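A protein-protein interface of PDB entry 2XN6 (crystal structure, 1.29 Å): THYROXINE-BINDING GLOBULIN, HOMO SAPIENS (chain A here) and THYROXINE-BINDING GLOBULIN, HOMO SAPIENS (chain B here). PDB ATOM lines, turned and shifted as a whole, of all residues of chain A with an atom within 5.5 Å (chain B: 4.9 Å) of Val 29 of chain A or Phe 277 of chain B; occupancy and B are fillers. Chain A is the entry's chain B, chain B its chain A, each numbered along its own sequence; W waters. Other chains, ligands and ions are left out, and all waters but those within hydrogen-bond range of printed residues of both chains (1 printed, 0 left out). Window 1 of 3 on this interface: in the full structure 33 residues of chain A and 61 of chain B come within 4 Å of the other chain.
ND2 of Asn 34 of chain B is in hydrogen-bond range of O of Asn 31 of chain A (2.9 Å). OD1 of Asn 34 of chain B is in hydrogen-bond range of N of Val 30 of chain A (2.7 Å).
ND1 of His 325 of chain B sits at hydrogen-bond distance from OG of Ser 278 of chain B, 2.8 Å away. The backbone carbonyl oxygen (O) of Gly 27 of chain A lies within hydrogen-bond range of the backbone NH (N) of Leu 13 of chain A (2.9 Å). O of Phe 277 of chain B sits at hydrogen-bond distance from N of Ile 326 of chain B (2.9 Å). The backbone carbonyl oxygen (O) of Ile 279 of chain B is in hydrogen-bond range of the backbone NH (N) of Leu 324 of chain B. The backbone carbonyl oxygen (O) of Phe 277 of chain B sits at hydrogen-bond distance from a ring nitrogen (ND1) of His 325 of chain B (3.4 Å). O of Phe 11 of chain A lies within hydrogen-bond range of N of Val 29 of chain A (2.8 Å).
Arg 9 of chain A touches Phe 194 of chain B (O to CZ, 3.2 Å). Phe 11 of chain A touches Phe 194 of chain B. Leu 324 of chain B touches Leu 13 of chain A (CD2 to CD2, 3.5 Å). Leu 13 of chain A touches Ile 326 of chain B. CA of Asn 34 of chain B touches O of Lys 28 of chain A (3.3 Å). Val 29 of chain A touches Asn 34 of chain B (C to OD1, 3.7 Å). Phe 194 of chain B touches Val 30 of chain A. Pro 32 of chain A touches Phe 194 of chain B. Ser 278 of chain B touches Pro 32 of chain A (O to O, 3.5 Å). O of Pro 32 of chain A touches CG2 of Ile 279 of chain B, at 3.97 Å.
Of chain B, only Asn 34 (3.7 Å) and Phe 277 (3.7 Å) come within 4 Å of Val 29 of chain A. Printed residues of chain A within 4 Å of Ile 326 of chain B: Leu 13 (3.9 Å). Of the printed residues of chain A, Phe 194 of chain B touches Arg 9 (3.2 Å), Ser 10 (3.9 Å), Phe 11 (3.9 Å), Val 30 (3.5 Å) and Pro 32 (3.5 Å). Of the printed residues of chain B, Val 30 of chain A touches Asn 34 and Phe 194. Of the printed residues of chain B, Leu 13 of chain A touches Leu 324 and Ile 326. Pro 275 of chain B touches none of the printed residues of chain A. The nearest residue of chain B that does not touch Val 29 of chain A is Ile 279 of chain B (4.1 Å). The nearest printed residue of chain B that does not touch Arg 9 of chain A is Pro 275 of chain B (7.0 Å).
Of the 11 printed residues of chain A, 9 touch a printed residue of chain B. Hydrophobic or aromatic side chains of chain A within 4 Å of the printed part of chain B: Phe 11, Leu 13, Val 29, Val 30 and Pro 32. Along chain B the printed residues that touch a printed residue of chain A span positions 34 to 326. Among the printed residues, 16 pairs touch across the chains. Among the printed residues, no Asp or Glu carboxylate lies within 4 Å of a Lys or Arg side-chain nitrogen of the other chain.
Water W1 lies within hydrogen-bond range of the backbone carbonyl oxygen of Pro 32 of chain A (2.7 Å) and the backbone NH of Ser 278 of chain B (3.0 Å).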
ATOM      1  N   ARG A   9     -30.078  19.379  20.372  1.00  0.00           N
ATOM      2  CA  ARG A   9     -28.964  19.227  19.453  1.00  0.00           C
ATOM      3  C   ARG A   9     -28.500  20.617  19.044  1.00  0.00           C
ATOM      4  O   ARG A   9     -29.088  21.619  19.473  1.00  0.00           O
ATOM      5  CB  ARG A   9     -29.357  18.388  18.227  1.00  0.00           C
ATOM      6  CG  ARG A   9     -30.473  18.959  17.395  1.00  0.00           C
ATOM      7  CD  ARG A   9     -30.717  18.159  16.122  1.00  0.00           C
ATOM      8  NE  ARG A   9     -31.765  18.783  15.318  1.00  0.00           N
ATOM      9  CZ  ARG A   9     -33.071  18.674  15.556  1.00  0.00           C
ATOM     10  NH1 ARG A   9     -33.526  17.940  16.568  1.00  0.00           N
ATOM     11  NH2 ARG A   9     -33.935  19.300  14.768  1.00  0.00           N
ATOM     12  N   SER A  10     -27.451  20.681  18.235  1.00  0.00           N
ATOM     13  CA  SER A  10     -26.817  21.956  17.883  1.00  0.00           C
ATOM     14  C   SER A  10     -27.814  23.012  17.436  1.00  0.00           C
ATOM     15  O   SER A  10     -28.693  22.750  16.620  1.00  0.00           O
ATOM     16  CB  SER A  10     -25.798  21.754  16.767  1.00  0.00           C
ATOM     17  OG  SER A  10     -24.682  21.022  17.218  1.00  0.00           O
ATOM     18  N   PHE A  11     -27.651  24.223  17.956  1.00  0.00           N
ATOM     19  CA  PHE A  11     -28.544  25.321  17.615  1.00  0.00           C
ATOM     20  C   PHE A  11     -27.768  26.621  17.564  1.00  0.00           C
ATOM     21  O   PHE A  11     -26.721  26.760  18.201  1.00  0.00           O
ATOM     22  CB  PHE A  11     -29.704  25.413  18.608  1.00  0.00           C
ATOM     23  CG  PHE A  11     -29.294  25.706  20.024  1.00  0.00           C
ATOM     24  CD1 PHE A  11     -28.932  24.688  20.895  1.00  0.00           C
ATOM     25  CD2 PHE A  11     -29.334  26.998  20.503  1.00  0.00           C
ATOM     26  CE1 PHE A  11     -28.593  24.958  22.206  1.00  0.00           C
ATOM     27  CE2 PHE A  11     -28.996  27.276  21.806  1.00  0.00           C
ATOM     28  CZ  PHE A  11     -28.625  26.252  22.664  1.00  0.00           C
ATOM     29  N   MET A  12     -28.268  27.574  16.785  1.00  0.00           N
ATOM     30  CA  MET A  12     -27.777  28.951  16.829  1.00  0.00           C
ATOM     31  C   MET A  12     -28.628  29.773  17.790  1.00  0.00           C
ATOM     32  O   MET A  12     -29.815  29.497  18.012  1.00  0.00           O
ATOM     33  CB  MET A  12     -27.775  29.584  15.439  1.00  0.00           C
ATOM     34  CG  MET A  12     -26.656  29.081  14.518  1.00  0.00           C
ATOM     35  SD  MET A  12     -26.607  29.883  12.898  1.00  0.00           S
ATOM     36  CE  MET A  12     -26.044  31.518  13.349  1.00  0.00           C
ATOM     37  N   LEU A  13     -28.006  30.799  18.355  1.00  0.00           N
ATOM     38  CA  LEU A  13     -28.638  31.670  19.325  1.00  0.00           C
ATOM     39  C   LEU A  13     -28.334  33.114  18.989  1.00  0.00           C
ATOM     40  O   LEU A  13     -27.182  33.448  18.701  1.00  0.00           O
ATOM     41  CB  LEU A  13     -28.084  31.371  20.718  1.00  0.00           C
ATOM     42  CG  LEU A  13     -28.538  32.245  21.886  1.00  0.00           C
ATOM     43  CD1 LEU A  13     -30.036  32.052  22.132  1.00  0.00           C
ATOM     44  CD2 LEU A  13     -27.732  31.979  23.161  1.00  0.00           C
ATOM     45  N   GLY A  27     -24.296  33.269  18.522  1.00  0.00           N
ATOM     46  CA  GLY A  27     -23.497  32.083  18.704  1.00  0.00           C
ATOM     47  C   GLY A  27     -24.112  30.818  18.164  1.00  0.00           C
ATOM     48  O   GLY A  27     -25.228  30.812  17.637  1.00  0.00           O
ATOM     49  N   LYS A  28     -23.343  29.753  18.301  1.00  0.00           N
ATOM     50  CA  LYS A  28     -23.788  28.403  18.010  1.00  0.00           C
ATOM     51  C   LYS A  28     -23.376  27.543  19.181  1.00  0.00           C
ATOM     52  O   LYS A  28     -22.216  27.560  19.605  1.00  0.00           O
ATOM     53  CB  LYS A  28     -23.142  27.872  16.746  1.00  0.00           C
ATOM     54  CG  LYS A  28     -23.461  26.399  16.465  1.00  0.00           C
ATOM     55  CD  LYS A  28     -22.978  25.942  15.096  1.00  0.00           C
ATOM     56  CE  LYS A  28     -21.480  26.168  14.906  1.00  0.00           C
ATOM     57  NZ  LYS A  28     -20.972  25.607  13.621  1.00  0.00           N
ATOM     58  N   VAL A  29     -24.328  26.782  19.694  1.00  0.00           N
ATOM     59  CA  VAL A  29     -24.071  25.860  20.788  1.00  0.00           C
ATOM     60  C   VAL A  29     -24.029  24.458  20.209  1.00  0.00           C
ATOM     61  O   VAL A  29     -25.052  23.928  19.792  1.00  0.00           O
ATOM     62  CB  VAL A  29     -25.151  25.961  21.875  1.00  0.00           C
ATOM     63  CG1 VAL A  29     -24.897  24.958  22.969  1.00  0.00           C
ATOM     64  CG2 VAL A  29     -25.194  27.368  22.445  1.00  0.00           C
ATOM     65  N   VAL A  30     -22.822  23.899  20.154  1.00  0.00           N
ATOM     66  CA  VAL A  30     -22.580  22.531  19.697  1.00  0.00           C
ATOM     67  C   VAL A  30     -22.500  21.580  20.892  1.00  0.00           C
ATOM     68  O   VAL A  30     -23.069  20.486  20.855  1.00  0.00           O
ATOM     69  CB  VAL A  30     -21.272  22.450  18.877  1.00  0.00           C
ATOM     70  CG1 VAL A  30     -20.940  21.007  18.517  1.00  0.00           C
ATOM     71  CG2 VAL A  30     -21.382  23.303  17.614  1.00  0.00           C
ATOM     72  N   ASN A  31     -21.768  21.988  21.925  1.00  0.00           N
ATOM     73  CA  ASN A  31     -21.642  21.215  23.158  1.00  0.00           C
ATOM     74  C   ASN A  31     -21.833  22.153  24.357  1.00  0.00           C
ATOM     75  O   ASN A  31     -20.914  22.895  24.724  1.00  0.00           O
ATOM     76  CB  ASN A  31     -20.280  20.521  23.226  1.00  0.00           C
ATOM     77  CG  ASN A  31     -20.129  19.659  24.468  1.00  0.00           C
ATOM     78  OD1 ASN A  31     -20.993  19.655  25.341  1.00  0.00           O
ATOM     79  ND2 ASN A  31     -19.031  18.923  24.549  1.00  0.00           N
ATOM     80  N   PRO A  32     -23.015  22.107  24.994  1.00  0.00           N
ATOM     81  CA  PRO A  32     -23.306  23.041  26.079  1.00  0.00           C
ATOM     82  C   PRO A  32     -22.541  22.795  27.376  1.00  0.00           C
ATOM     83  O   PRO A  32     -22.604  23.636  28.269  1.00  0.00           O
ATOM     84  CB  PRO A  32     -24.811  22.859  26.298  1.00  0.00           C
ATOM     85  CG  PRO A  32     -25.096  21.493  25.820  1.00  0.00           C
ATOM     86  CD  PRO A  32     -24.171  21.245  24.687  1.00  0.00           C
ATOM     87  N   ASN B  34     -18.399  25.303  19.509  1.00  0.00           N
ATOM     88  CA  ASN B  34     -19.152  26.420  20.051  1.00  0.00           C
ATOM     89  C   ASN B  34     -18.600  27.746  19.542  1.00  0.00           C
ATOM     90  O   ASN B  34     -17.379  27.924  19.461  1.00  0.00           O
ATOM     91  CB  ASN B  34     -19.069  26.457  21.582  1.00  0.00           C
ATOM     92  CG  ASN B  34     -19.806  25.314  22.258  1.00  0.00           C
ATOM     93  OD1 ASN B  34     -20.657  24.651  21.665  1.00  0.00           O
ATOM     94  ND2 ASN B  34     -19.477  25.087  23.528  1.00  0.00           N
ATOM     95  N   PHE B 194     -28.211  15.607  25.158  1.00  0.00           N
ATOM     96  CA  PHE B 194     -28.059  16.633  24.148  1.00  0.00           C
ATOM     97  C   PHE B 194     -27.075  16.076  23.140  1.00  0.00           C
ATOM     98  O   PHE B 194     -25.972  15.684  23.506  1.00  0.00           O
ATOM     99  CB  PHE B 194     -27.529  17.913  24.786  1.00  0.00           C
ATOM    100  CG  PHE B 194     -27.456  19.083  23.845  1.00  0.00           C
ATOM    101  CD1 PHE B 194     -28.415  20.081  23.888  1.00  0.00           C
ATOM    102  CD2 PHE B 194     -26.418  19.189  22.934  1.00  0.00           C
ATOM    103  CE1 PHE B 194     -28.343  21.168  23.027  1.00  0.00           C
ATOM    104  CE2 PHE B 194     -26.341  20.271  22.071  1.00  0.00           C
ATOM    105  CZ  PHE B 194     -27.304  21.263  22.121  1.00  0.00           C
ATOM    106  N   PRO B 275     -31.992  23.731  27.189  1.00  0.00           N
ATOM    107  CA  PRO B 275     -30.961  23.412  28.178  1.00  0.00           C
ATOM    108  C   PRO B 275     -30.581  24.599  29.056  1.00  0.00           C
ATOM    109  O   PRO B 275     -30.661  25.751  28.621  1.00  0.00           O
ATOM    110  CB  PRO B 275     -29.769  23.009  27.316  1.00  0.00           C
ATOM    111  CG  PRO B 275     -29.959  23.785  26.064  1.00  0.00           C
ATOM    112  CD  PRO B 275     -31.442  23.752  25.827  1.00  0.00           C
ATOM    113  N   LYS B 276     -30.178  24.285  30.283  1.00  0.00           N
ATOM    114  CA  LYS B 276     -29.555  25.230  31.196  1.00  0.00           C
ATOM    115  C   LYS B 276     -28.062  25.025  31.066  1.00  0.00           C
ATOM    116  O   LYS B 276     -27.584  23.908  31.247  1.00  0.00           O
ATOM    117  CB  LYS B 276     -30.010  24.932  32.624  1.00  0.00           C
ATOM    118  CG  LYS B 276     -29.355  25.776  33.692  1.00  0.00           C
ATOM    119  CD  LYS B 276     -30.048  25.574  35.024  1.00  0.00           C
ATOM    120  CE  LYS B 276     -29.449  26.413  36.125  1.00  0.00           C
ATOM    121  NZ  LYS B 276     -30.159  26.190  37.412  1.00  0.00           N
ATOM    122  N   PHE B 277     -27.323  26.079  30.740  1.00  0.00           N
ATOM    123  CA  PHE B 277     -25.905  25.913  30.450  1.00  0.00           C
ATOM    124  C   PHE B 277     -25.160  27.234  30.447  1.00  0.00           C
ATOM    125  O   PHE B 277     -25.754  28.308  30.454  1.00  0.00           O
ATOM    126  CB  PHE B 277     -25.737  25.242  29.077  1.00  0.00           C
ATOM    127  CG  PHE B 277     -26.125  26.121  27.931  1.00  0.00           C
ATOM    128  CD1 PHE B 277     -25.157  26.755  27.163  1.00  0.00           C
ATOM    129  CD2 PHE B 277     -27.459  26.351  27.629  1.00  0.00           C
ATOM    130  CE1 PHE B 277     -25.507  27.597  26.120  1.00  0.00           C
ATOM    131  CE2 PHE B 277     -27.809  27.182  26.592  1.00  0.00           C
ATOM    132  CZ  PHE B 277     -26.824  27.812  25.825  1.00  0.00           C
ATOM    133  N   SER B 278     -23.836  27.118  30.444  1.00  0.00           N
ATOM    134  CA  SER B 278     -22.941  28.253  30.281  1.00  0.00           C
ATOM    135  C   SER B 278     -21.862  27.881  29.297  1.00  0.00           C
ATOM    136  O   SER B 278     -21.366  26.748  29.321  1.00  0.00           O
ATOM    137  CB  SER B 278     -22.242  28.596  31.593  1.00  0.00           C
ATOM    138  OG  SER B 278     -23.146  28.766  32.660  1.00  0.00           O
ATOM    139  N   ILE B 279     -21.479  28.833  28.453  1.00  0.00           N
ATOM    140  CA  ILE B 279     -20.299  28.664  27.609  1.00  0.00           C
ATOM    141  C   ILE B 279     -19.513  29.966  27.526  1.00  0.00           C
ATOM    142  O   ILE B 279     -19.971  31.036  27.945  1.00  0.00           O
ATOM    143  CB  ILE B 279     -20.646  28.167  26.192  1.00  0.00           C
ATOM    144  CG1 ILE B 279     -21.637  29.115  25.519  1.00  0.00           C
ATOM    145  CG2 ILE B 279     -21.214  26.749  26.239  1.00  0.00           C
ATOM    146  CD1 ILE B 279     -21.709  28.953  24.003  1.00  0.00           C
ATOM    147  N   LEU B 324     -21.656  33.439  28.306  1.00  0.00           N
ATOM    148  CA  LEU B 324     -23.104  33.286  28.298  1.00  0.00           C
ATOM    149  C   LEU B 324     -23.529  32.328  29.390  1.00  0.00           C
ATOM    150  O   LEU B 324     -22.952  31.257  29.512  1.00  0.00           O
ATOM    151  CB  LEU B 324     -23.541  32.672  26.959  1.00  0.00           C
ATOM    152  CG  LEU B 324     -25.006  32.267  26.786  1.00  0.00           C
ATOM    153  CD1 LEU B 324     -25.884  33.484  26.786  1.00  0.00           C
ATOM    154  CD2 LEU B 324     -25.154  31.480  25.499  1.00  0.00           C
ATOM    155  N   HIS B 325     -24.580  32.685  30.126  1.00  0.00           N
ATOM    156  CA  HIS B 325     -25.299  31.740  30.977  1.00  0.00           C
ATOM    157  C   HIS B 325     -26.792  31.844  30.726  1.00  0.00           C
ATOM    158  O   HIS B 325     -27.351  32.941  30.735  1.00  0.00           O
ATOM    159  CB  HIS B 325     -25.039  31.970  32.464  1.00  0.00           C
ATOM    160  CG  HIS B 325     -25.879  31.095  33.342  1.00  0.00           C
ATOM    161  ND1 HIS B 325     -25.635  29.747  33.500  1.00  0.00           N
ATOM    162  CD2 HIS B 325     -27.006  31.357  34.043  1.00  0.00           C
ATOM    163  CE1 HIS B 325     -26.551  29.226  34.298  1.00  0.00           C
ATOM    164  NE2 HIS B 325     -27.391  30.184  34.646  1.00  0.00           N
ATOM    165  N   ILE B 326     -27.426  30.694  30.524  1.00  0.00           N
ATOM    166  CA  ILE B 326     -28.879  30.598  30.405  1.00  0.00           C
ATOM    167  C   ILE B 326     -29.404  29.651  31.474  1.00  0.00           C
ATOM    168  O   ILE B 326     -28.916  28.530  31.611  1.00  0.00           O
ATOM    169  CB  ILE B 326     -29.286  30.087  29.004  1.00  0.00           C
ATOM    170  CG1 ILE B 326     -29.125  31.228  27.994  1.00  0.00           C
ATOM    171  CG2 ILE B 326     -30.719  29.536  29.009  1.00  0.00           C
ATOM    172  CD1 ILE B 326     -29.314  30.839  26.554  1.00  0.00           C
HETATM  173  O   HOH W   1     -22.910  24.278  30.859  1.00  0.00           O
